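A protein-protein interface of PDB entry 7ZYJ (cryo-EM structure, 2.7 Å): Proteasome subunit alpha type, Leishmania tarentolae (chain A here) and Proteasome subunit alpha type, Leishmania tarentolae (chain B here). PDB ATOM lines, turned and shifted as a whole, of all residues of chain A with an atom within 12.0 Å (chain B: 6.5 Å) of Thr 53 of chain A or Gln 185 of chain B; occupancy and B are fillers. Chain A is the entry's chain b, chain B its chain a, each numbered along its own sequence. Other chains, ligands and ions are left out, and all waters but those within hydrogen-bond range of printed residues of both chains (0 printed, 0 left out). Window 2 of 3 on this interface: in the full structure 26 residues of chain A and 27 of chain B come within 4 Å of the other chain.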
ATOM      1  N   LYS A  48     -20.106  10.751  -2.428  1.00  0.00           N
ATOM      2  CA  LYS A  48     -19.850  10.607  -3.862  1.00  0.00           C
ATOM      3  C   LYS A  48     -21.163  10.278  -4.567  1.00  0.00           C
ATOM      4  O   LYS A  48     -21.466   9.128  -4.891  1.00  0.00           O
ATOM      5  CB  LYS A  48     -18.800   9.536  -4.124  1.00  0.00           C
ATOM      6  CG  LYS A  48     -17.537   9.665  -3.299  1.00  0.00           C
ATOM      7  CD  LYS A  48     -16.461   8.722  -3.815  1.00  0.00           C
ATOM      8  CE  LYS A  48     -17.015   7.328  -4.063  1.00  0.00           C
ATOM      9  NZ  LYS A  48     -15.939   6.355  -4.405  1.00  0.00           N
ATOM     10  N   LYS A  49     -21.951  11.320  -4.817  1.00  0.00           N
ATOM     11  CA  LYS A  49     -23.211  11.179  -5.539  1.00  0.00           C
ATOM     12  C   LYS A  49     -22.956  11.491  -7.008  1.00  0.00           C
ATOM     13  O   LYS A  49     -22.894  12.660  -7.403  1.00  0.00           O
ATOM     14  CB  LYS A  49     -24.278  12.098  -4.949  1.00  0.00           C
ATOM     15  CG  LYS A  49     -25.668  11.886  -5.526  1.00  0.00           C
ATOM     16  CD  LYS A  49     -26.037  12.982  -6.512  1.00  0.00           C
ATOM     17  CE  LYS A  49     -26.329  14.289  -5.795  1.00  0.00           C
ATOM     18  NZ  LYS A  49     -26.809  15.341  -6.731  1.00  0.00           N
ATOM     19  N   ALA A  50     -22.804  10.444  -7.814  1.00  0.00           N
ATOM     20  CA  ALA A  50     -22.518  10.623  -9.226  1.00  0.00           C
ATOM     21  C   ALA A  50     -23.736  11.195  -9.949  1.00  0.00           C
ATOM     22  O   ALA A  50     -24.878  10.928  -9.566  1.00  0.00           O
ATOM     23  CB  ALA A  50     -22.113   9.296  -9.861  1.00  0.00           C
ATOM     24  N   PRO A  51     -23.518  11.996 -10.995  1.00  0.00           N
ATOM     25  CA  PRO A  51     -24.659  12.538 -11.752  1.00  0.00           C
ATOM     26  C   PRO A  51     -25.526  11.469 -12.393  1.00  0.00           C
ATOM     27  O   PRO A  51     -26.718  11.712 -12.617  1.00  0.00           O
ATOM     28  CB  PRO A  51     -23.992  13.425 -12.814  1.00  0.00           C
ATOM     29  CG  PRO A  51     -22.617  13.697 -12.291  1.00  0.00           C
ATOM     30  CD  PRO A  51     -22.228  12.489 -11.503  1.00  0.00           C
ATOM     31  N   SER A  52     -24.971  10.298 -12.694  1.00  0.00           N
ATOM     32  CA  SER A  52     -25.720   9.226 -13.331  1.00  0.00           C
ATOM     33  C   SER A  52     -25.168   7.891 -12.849  1.00  0.00           C
ATOM     34  O   SER A  52     -24.182   7.832 -12.110  1.00  0.00           O
ATOM     35  CB  SER A  52     -25.653   9.340 -14.857  1.00  0.00           C
ATOM     36  OG  SER A  52     -26.275   8.229 -15.477  1.00  0.00           O
ATOM     37  N   THR A  53     -25.826   6.810 -13.263  1.00  0.00           N
ATOM     38  CA  THR A  53     -25.327   5.471 -12.986  1.00  0.00           C
ATOM     39  C   THR A  53     -24.258   5.029 -13.975  1.00  0.00           C
ATOM     40  O   THR A  53     -23.674   3.955 -13.795  1.00  0.00           O
ATOM     41  CB  THR A  53     -26.480   4.464 -12.993  1.00  0.00           C
ATOM     42  OG1 THR A  53     -27.127   4.486 -14.270  1.00  0.00           O
ATOM     43  CG2 THR A  53     -27.492   4.810 -11.912  1.00  0.00           C
ATOM     44  N   LEU A  54     -23.992   5.829 -15.008  1.00  0.00           N
ATOM     45  CA  LEU A  54     -22.986   5.531 -16.020  1.00  0.00           C
ATOM     46  C   LEU A  54     -21.691   6.301 -15.789  1.00  0.00           C
ATOM     47  O   LEU A  54     -20.977   6.616 -16.747  1.00  0.00           O
ATOM     48  CB  LEU A  54     -23.540   5.839 -17.410  1.00  0.00           C
ATOM     49  CG  LEU A  54     -24.744   5.022 -17.871  1.00  0.00           C
ATOM     50  CD1 LEU A  54     -25.395   5.693 -19.060  1.00  0.00           C
ATOM     51  CD2 LEU A  54     -24.321   3.609 -18.224  1.00  0.00           C
ATOM     52  N   VAL A  55     -21.372   6.610 -14.534  1.00  0.00           N
ATOM     53  CA  VAL A  55     -20.243   7.467 -14.197  1.00  0.00           C
ATOM     54  C   VAL A  55     -19.067   6.681 -13.634  1.00  0.00           C
ATOM     55  O   VAL A  55     -17.972   7.243 -13.486  1.00  0.00           O
ATOM     56  CB  VAL A  55     -20.680   8.585 -13.225  1.00  0.00           C
ATOM     57  CG1 VAL A  55     -19.573   9.605 -12.979  1.00  0.00           C
ATOM     58  CG2 VAL A  55     -21.913   9.287 -13.766  1.00  0.00           C
ATOM     59  N   ASP A  56     -19.241   5.387 -13.354  1.00  0.00           N
ATOM     60  CA  ASP A  56     -18.162   4.544 -12.837  1.00  0.00           C
ATOM     61  C   ASP A  56     -17.607   5.128 -11.534  1.00  0.00           C
ATOM     62  O   ASP A  56     -16.478   5.615 -11.457  1.00  0.00           O
ATOM     63  CB  ASP A  56     -17.059   4.358 -13.888  1.00  0.00           C
ATOM     64  CG  ASP A  56     -15.969   3.410 -13.428  1.00  0.00           C
ATOM     65  OD1 ASP A  56     -16.254   2.534 -12.586  1.00  0.00           O
ATOM     66  OD2 ASP A  56     -14.824   3.544 -13.908  1.00  0.00           O
ATOM     67  N   ALA A  57     -18.466   5.084 -10.509  1.00  0.00           N
ATOM     68  CA  ALA A  57     -18.203   5.744  -9.234  1.00  0.00           C
ATOM     69  C   ALA A  57     -16.832   5.422  -8.649  1.00  0.00           C
ATOM     70  O   ALA A  57     -16.346   6.167  -7.792  1.00  0.00           O
ATOM     71  CB  ALA A  57     -19.289   5.368  -8.223  1.00  0.00           C
ATOM     72  N   SER A  58     -16.197   4.330  -9.079  1.00  0.00           N
ATOM     73  CA  SER A  58     -14.840   4.047  -8.632  1.00  0.00           C
ATOM     74  C   SER A  58     -13.833   5.056  -9.170  1.00  0.00           C
ATOM     75  O   SER A  58     -12.770   5.232  -8.567  1.00  0.00           O
ATOM     76  CB  SER A  58     -14.432   2.634  -9.051  1.00  0.00           C
ATOM     77  OG  SER A  58     -13.858   2.633 -10.346  1.00  0.00           O
ATOM     78  N   SER A  59     -14.143   5.720 -10.284  1.00  0.00           N
ATOM     79  CA  SER A  59     -13.233   6.694 -10.872  1.00  0.00           C
ATOM     80  C   SER A  59     -13.320   8.064 -10.216  1.00  0.00           C
ATOM     81  O   SER A  59     -12.342   8.819 -10.250  1.00  0.00           O
ATOM     82  CB  SER A  59     -13.510   6.835 -12.370  1.00  0.00           C
ATOM     83  OG  SER A  59     -14.584   7.727 -12.604  1.00  0.00           O
ATOM     84  N   ILE A  60     -14.460   8.406  -9.623  1.00  0.00           N
ATOM     85  CA  ILE A  60     -14.636   9.700  -8.973  1.00  0.00           C
ATOM     86  C   ILE A  60     -14.232   9.570  -7.511  1.00  0.00           C
ATOM     87  O   ILE A  60     -14.633   8.626  -6.822  1.00  0.00           O
ATOM     88  CB  ILE A  60     -16.084  10.205  -9.117  1.00  0.00           C
ATOM     89  CG1 ILE A  60     -17.087   9.182  -8.582  1.00  0.00           C
ATOM     90  CG2 ILE A  60     -16.389  10.539 -10.569  1.00  0.00           C
ATOM     91  CD1 ILE A  60     -18.527   9.631  -8.687  1.00  0.00           C
ATOM     92  N   GLN A 200     -30.279   6.158  -0.390  1.00  0.00           N
ATOM     93  CA  GLN A 200     -29.678   5.101   0.411  1.00  0.00           C
ATOM     94  C   GLN A 200     -28.167   5.117   0.228  1.00  0.00           C
ATOM     95  O   GLN A 200     -27.675   5.209  -0.901  1.00  0.00           O
ATOM     96  CB  GLN A 200     -30.243   3.734   0.024  1.00  0.00           C
ATOM     97  CG  GLN A 200     -29.654   2.574   0.808  1.00  0.00           C
ATOM     98  CD  GLN A 200     -29.977   2.648   2.287  1.00  0.00           C
ATOM     99  OE1 GLN A 200     -31.099   2.974   2.674  1.00  0.00           O
ATOM    100  NE2 GLN A 200     -28.991   2.343   3.123  1.00  0.00           N
ATOM    101  N   THR A 202     -24.828   3.519  -0.215  1.00  0.00           N
ATOM    102  CA  THR A 202     -24.156   2.297  -0.628  1.00  0.00           C
ATOM    103  C   THR A 202     -22.649   2.508  -0.579  1.00  0.00           C
ATOM    104  O   THR A 202     -22.156   3.636  -0.513  1.00  0.00           O
ATOM    105  CB  THR A 202     -24.597   1.874  -2.034  1.00  0.00           C
ATOM    106  OG1 THR A 202     -24.308   2.924  -2.964  1.00  0.00           O
ATOM    107  CG2 THR A 202     -26.089   1.581  -2.057  1.00  0.00           C
ATOM    108  N   GLU A 204     -20.608   2.227  -2.871  1.00  0.00           N
ATOM    109  CA  GLU A 204     -20.187   2.963  -4.053  1.00  0.00           C
ATOM    110  C   GLU A 204     -20.681   4.402  -4.046  1.00  0.00           C
ATOM    111  O   GLU A 204     -20.316   5.175  -4.936  1.00  0.00           O
ATOM    112  CB  GLU A 204     -20.667   2.261  -5.332  1.00  0.00           C
ATOM    113  CG  GLU A 204     -20.184   0.821  -5.530  1.00  0.00           C
ATOM    114  CD  GLU A 204     -20.764  -0.160  -4.528  1.00  0.00           C
ATOM    115  OE1 GLU A 204     -21.996  -0.369  -4.544  1.00  0.00           O
ATOM    116  OE2 GLU A 204     -19.991  -0.720  -3.722  1.00  0.00           O
ATOM    117  N   ASN A 205     -21.502   4.775  -3.063  1.00  0.00           N
ATOM    118  CA  ASN A 205     -22.020   6.130  -2.946  1.00  0.00           C
ATOM    119  C   ASN A 205     -21.259   6.977  -1.937  1.00  0.00           C
ATOM    120  O   ASN A 205     -21.400   8.204  -1.950  1.00  0.00           O
ATOM    121  CB  ASN A 205     -23.502   6.095  -2.553  1.00  0.00           C
ATOM    122  CG  ASN A 205     -24.318   7.161  -3.252  1.00  0.00           C
ATOM    123  OD1 ASN A 205     -23.793   8.197  -3.653  1.00  0.00           O
ATOM    124  ND2 ASN A 205     -25.614   6.912  -3.400  1.00  0.00           N
ATOM    125  N   ILE B 166     -18.608   4.466 -17.587  1.00  0.00           N
ATOM    126  CA  ILE B 166     -19.010   3.238 -18.262  1.00  0.00           C
ATOM    127  C   ILE B 166     -19.579   3.547 -19.639  1.00  0.00           C
ATOM    128  O   ILE B 166     -19.269   2.863 -20.617  1.00  0.00           O
ATOM    129  CB  ILE B 166     -20.020   2.465 -17.391  1.00  0.00           C
ATOM    130  CG1 ILE B 166     -19.380   2.066 -16.061  1.00  0.00           C
ATOM    131  CG2 ILE B 166     -20.534   1.240 -18.128  1.00  0.00           C
ATOM    132  CD1 ILE B 166     -20.352   1.477 -15.068  1.00  0.00           C
ATOM    133  N   PHE B 180     -31.380   7.515 -22.758  1.00  0.00           N
ATOM    134  CA  PHE B 180     -31.506   6.243 -23.464  1.00  0.00           C
ATOM    135  C   PHE B 180     -30.495   5.228 -22.943  1.00  0.00           C
ATOM    136  O   PHE B 180     -30.829   4.058 -22.718  1.00  0.00           O
ATOM    137  CB  PHE B 180     -31.330   6.464 -24.968  1.00  0.00           C
ATOM    138  CG  PHE B 180     -31.611   5.245 -25.804  1.00  0.00           C
ATOM    139  CD1 PHE B 180     -30.630   4.290 -26.019  1.00  0.00           C
ATOM    140  CD2 PHE B 180     -32.854   5.059 -26.382  1.00  0.00           C
ATOM    141  CE1 PHE B 180     -30.886   3.172 -26.788  1.00  0.00           C
ATOM    142  CE2 PHE B 180     -33.116   3.943 -27.153  1.00  0.00           C
ATOM    143  CZ  PHE B 180     -32.130   2.999 -27.356  1.00  0.00           C
ATOM    144  N   LEU B 181     -29.246   5.662 -22.748  1.00  0.00           N
ATOM    145  CA  LEU B 181     -28.220   4.756 -22.243  1.00  0.00           C
ATOM    146  C   LEU B 181     -28.540   4.287 -20.828  1.00  0.00           C
ATOM    147  O   LEU B 181     -28.338   3.113 -20.498  1.00  0.00           O
ATOM    148  CB  LEU B 181     -26.851   5.433 -22.293  1.00  0.00           C
ATOM    149  CG  LEU B 181     -26.271   5.716 -23.681  1.00  0.00           C
ATOM    150  CD1 LEU B 181     -25.147   6.735 -23.595  1.00  0.00           C
ATOM    151  CD2 LEU B 181     -25.785   4.432 -24.332  1.00  0.00           C
ATOM    152  N   GLU B 182     -29.036   5.188 -19.976  1.00  0.00           N
ATOM    153  CA  GLU B 182     -29.415   4.800 -18.621  1.00  0.00           C
ATOM    154  C   GLU B 182     -30.578   3.816 -18.633  1.00  0.00           C
ATOM    155  O   GLU B 182     -30.594   2.858 -17.851  1.00  0.00           O
ATOM    156  CB  GLU B 182     -29.772   6.038 -17.799  1.00  0.00           C
ATOM    157  CG  GLU B 182     -28.582   6.898 -17.410  1.00  0.00           C
ATOM    158  CD  GLU B 182     -28.956   8.355 -17.225  1.00  0.00           C
ATOM    159  OE1 GLU B 182     -30.130   8.633 -16.899  1.00  0.00           O
ATOM    160  OE2 GLU B 182     -28.078   9.224 -17.405  1.00  0.00           O
ATOM    161  N   LYS B 183     -31.567   4.044 -19.501  1.00  0.00           N
ATOM    162  CA  LYS B 183     -32.691   3.121 -19.603  1.00  0.00           C
ATOM    163  C   LYS B 183     -32.231   1.746 -20.069  1.00  0.00           C
ATOM    164  O   LYS B 183     -32.688   0.722 -19.550  1.00  0.00           O
ATOM    165  CB  LYS B 183     -33.749   3.683 -20.552  1.00  0.00           C
ATOM    166  CG  LYS B 183     -34.956   2.779 -20.738  1.00  0.00           C
ATOM    167  CD  LYS B 183     -36.037   3.462 -21.558  1.00  0.00           C
ATOM    168  CE  LYS B 183     -35.619   3.604 -23.012  1.00  0.00           C
ATOM    169  NZ  LYS B 183     -35.548   2.288 -23.701  1.00  0.00           N
ATOM    170  N   ARG B 184     -31.328   1.704 -21.051  1.00  0.00           N
ATOM    171  CA  ARG B 184     -30.800   0.422 -21.505  1.00  0.00           C
ATOM    172  C   ARG B 184     -29.952  -0.247 -20.429  1.00  0.00           C
ATOM    173  O   ARG B 184     -29.894  -1.480 -20.364  1.00  0.00           O
ATOM    174  CB  ARG B 184     -29.991   0.612 -22.787  1.00  0.00           C
ATOM    175  CG  ARG B 184     -29.510  -0.684 -23.416  1.00  0.00           C
ATOM    176  CD  ARG B 184     -30.679  -1.554 -23.850  1.00  0.00           C
ATOM    177  NE  ARG B 184     -31.517  -0.895 -24.843  1.00  0.00           N
ATOM    178  CZ  ARG B 184     -31.294  -0.923 -26.149  1.00  0.00           C
ATOM    179  NH1 ARG B 184     -30.264  -1.575 -26.661  1.00  0.00           N
ATOM    180  NH2 ARG B 184     -32.127  -0.281 -26.964  1.00  0.00           N
ATOM    181  N   GLN B 185     -29.300   0.543 -19.575  1.00  0.00           N
ATOM    182  CA  GLN B 185     -28.488  -0.007 -18.498  1.00  0.00           C
ATOM    183  C   GLN B 185     -29.322  -0.660 -17.404  1.00  0.00           C
ATOM    184  O   GLN B 185     -28.816  -1.544 -16.703  1.00  0.00           O
ATOM    185  CB  GLN B 185     -27.612   1.091 -17.890  1.00  0.00           C
ATOM    186  CG  GLN B 185     -26.543   0.586 -16.936  1.00  0.00           C
ATOM    187  CD  GLN B 185     -26.061   1.659 -15.982  1.00  0.00           C
ATOM    188  OE1 GLN B 185     -26.697   2.703 -15.833  1.00  0.00           O
ATOM    189  NE2 GLN B 185     -24.933   1.408 -15.330  1.00  0.00           N
ATOM    190  N   LYS B 186     -30.581  -0.250 -17.239  1.00  0.00           N
ATOM    191  CA  LYS B 186     -31.418  -0.823 -16.191  1.00  0.00           C
ATOM    192  C   LYS B 186     -31.714  -2.297 -16.424  1.00  0.00           C
ATOM    193  O   LYS B 186     -31.998  -3.021 -15.464  1.00  0.00           O
ATOM    194  CB  LYS B 186     -32.726  -0.040 -16.076  1.00  0.00           C
ATOM    195  CG  LYS B 186     -32.545   1.403 -15.640  1.00  0.00           C
ATOM    196  CD  LYS B 186     -33.882   2.095 -15.436  1.00  0.00           C
ATOM    197  CE  LYS B 186     -33.696   3.584 -15.199  1.00  0.00           C
ATOM    198  NZ  LYS B 186     -32.950   3.860 -13.940  1.00  0.00           N
ATOM    199  N   SER B 187     -31.657  -2.760 -17.674  1.00  0.00           N
ATOM    200  CA  SER B 187     -31.951  -4.150 -18.005  1.00  0.00           C
ATOM    201  C   SER B 187     -30.684  -4.991 -18.128  1.00  0.00           C
ATOM    202  O   SER B 187     -30.530  -5.992 -17.423  1.00  0.00           O
ATOM    203  CB  SER B 187     -32.765  -4.215 -19.305  1.00  0.00           C
ATOM    204  OG  SER B 187     -32.039  -3.661 -20.388  1.00  0.00           O
ATOM    205  N   THR B 188     -29.772  -4.598 -19.010  1.00  0.00           N
ATOM    206  CA  THR B 188     -28.552  -5.347 -19.261  1.00  0.00           C
ATOM    207  C   THR B 188     -27.408  -4.797 -18.412  1.00  0.00           C
ATOM    208  O   THR B 188     -27.559  -3.832 -17.659  1.00  0.00           O
ATOM    209  CB  THR B 188     -28.196  -5.305 -20.748  1.00  0.00           C
ATOM    210  OG1 THR B 188     -27.931  -3.952 -21.140  1.00  0.00           O
ATOM    211  CG2 THR B 188     -29.342  -5.853 -21.583  1.00  0.00           C
ATOM    212  N   GLU B 189     -26.243  -5.428 -18.538  1.00  0.00           N
ATOM    213  CA  GLU B 189     -25.024  -4.993 -17.863  1.00  0.00           C
ATOM    214  C   GLU B 189     -24.004  -4.647 -18.939  1.00  0.00           C
ATOM    215  O   GLU B 189     -23.539  -5.531 -19.666  1.00  0.00           O
ATOM    216  CB  GLU B 189     -24.499  -6.074 -16.920  1.00  0.00           C
ATOM    217  CG  GLU B 189     -23.734  -5.537 -15.721  1.00  0.00           C
ATOM    218  CD  GLU B 189     -22.304  -5.165 -16.057  1.00  0.00           C
ATOM    219  OE1 GLU B 189     -21.737  -5.772 -16.987  1.00  0.00           O
ATOM    220  OE2 GLU B 189     -21.749  -4.266 -15.391  1.00  0.00           O
ATOM    221  N   LEU B 190     -23.656  -3.362 -19.037  1.00  0.00           N
ATOM    222  CA  LEU B 190     -22.825  -2.893 -20.143  1.00  0.00           C
ATOM    223  C   LEU B 190     -21.421  -3.484 -20.085  1.00  0.00           C
ATOM    224  O   LEU B 190     -20.832  -3.796 -21.126  1.00  0.00           O
ATOM    225  CB  LEU B 190     -22.765  -1.366 -20.146  1.00  0.00           C
ATOM    226  CG  LEU B 190     -23.893  -0.614 -20.859  1.00  0.00           C
ATOM    227  CD1 LEU B 190     -25.223  -0.784 -20.146  1.00  0.00           C
ATOM    228  CD2 LEU B 190     -23.542   0.859 -20.994  1.00  0.00           C
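Hydrophobic or aromatic side chains of chain B within 4 Å of the printed part of chain A: Ile 166, Leu 181 and Leu 190.
Printed residues of chain A that touch a printed residue of chain B: Ser 52, Thr 53, Leu 54 and Asp 56.
Hydrophobic or aromatic side chains of chain A that line the printed part of chain B: Leu 54.
Among the printed residues, no Asp or Glu carboxylate lies within 4 Å of a Lys or Arg side-chain nitrogen of the other chain.
Of chain B, only Gln 185 (2.4 Å) comes within 4 Å of Thr 53 of chain A.
Of chain A, only Thr 53 (2.4 Å) and Leu 54 (3.4 Å) come within 4 Å of Gln 185 of chain B.
Of the printed residues of chain A, Ile 166 of chain B touches Leu 54 (3.3 Å) and Asp 56 (3.9 Å).
Of the printed residues of chain A, Glu 182 of chain B touches Ser 52 (2.8 Å) and Leu 54 (3.8 Å).
No residue of chain A comes within 4 Å of Lys 183 of chain B.
No residue of chain A comes within 4 Å of Lys 186 of chain B.
No residue of chain A comes within 4 Å of Thr 188 of chain B.
Of the printed residues of chain A, Leu 190 of chain B touches Leu 54.
Of the printed residues of chain B, Asp 56 of chain A touches Ile 166.
Of the printed residues of chain B, Ser 52 of chain A touches Glu 182 (2.8 Å).
Of the printed residues of chain B, Leu 54 of chain A touches Ile 166, Leu 181, Glu 182, Gln 185 and Leu 190.
Lys 48 of chain A touches none of the printed residues of chain B.
Phe 180 of chain B touches none of the printed residues of chain A.
The nearest residue of chain A that does not touch Gln 185 of chain B is Ser 52 of chain A (5.6 Å).
The nearest printed residue of chain B that does not touch Leu 54 of chain A is Lys 183 of chain B (6.4 Å).
Among the printed residues, pairs that only touch across the chains: Leu 54 of chain A with Gln 185 of chain B (3.4 Å), Leu 54 of chain A with Leu 181 of chain B (3.6 Å), Leu 54 of chain A with Glu 182 of chain B (3.8 Å), Asp 56 of chain A with Ile 166 of chain B (3.9 Å) and Leu 54 of chain A with Leu 190 of chain B (3.98 Å).
The side-chain hydroxyl of Ser 52 of chain A lies close to the backbone NH of Leu 54 of chain A, 3.3 Å away.
OG of Ser 58 of chain A lies within hydrogen-bond range of OD1 of Asp 56 of chain A (3.3 Å).
The side-chain hydroxyl (OG) of Ser 59 of chain A sits at hydrogen-bond distance from the backbone carbonyl oxygen (O) of Asp 56 of chain A (3.1 Å).
N of Ile 166 of chain B is in hydrogen-bond range of O of Leu 54 of chain A (3.3 Å).
OE1 of Gln 185 of chain B sits at hydrogen-bond distance from OG1 of Thr 53 of chain A (2.4 Å).
The side-chain carboxylate (OE2) of Glu 182 of chain B is in hydrogen-bond range of the side-chain hydroxyl (OG) of Ser 52 of chain A, at 2.8 Å.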
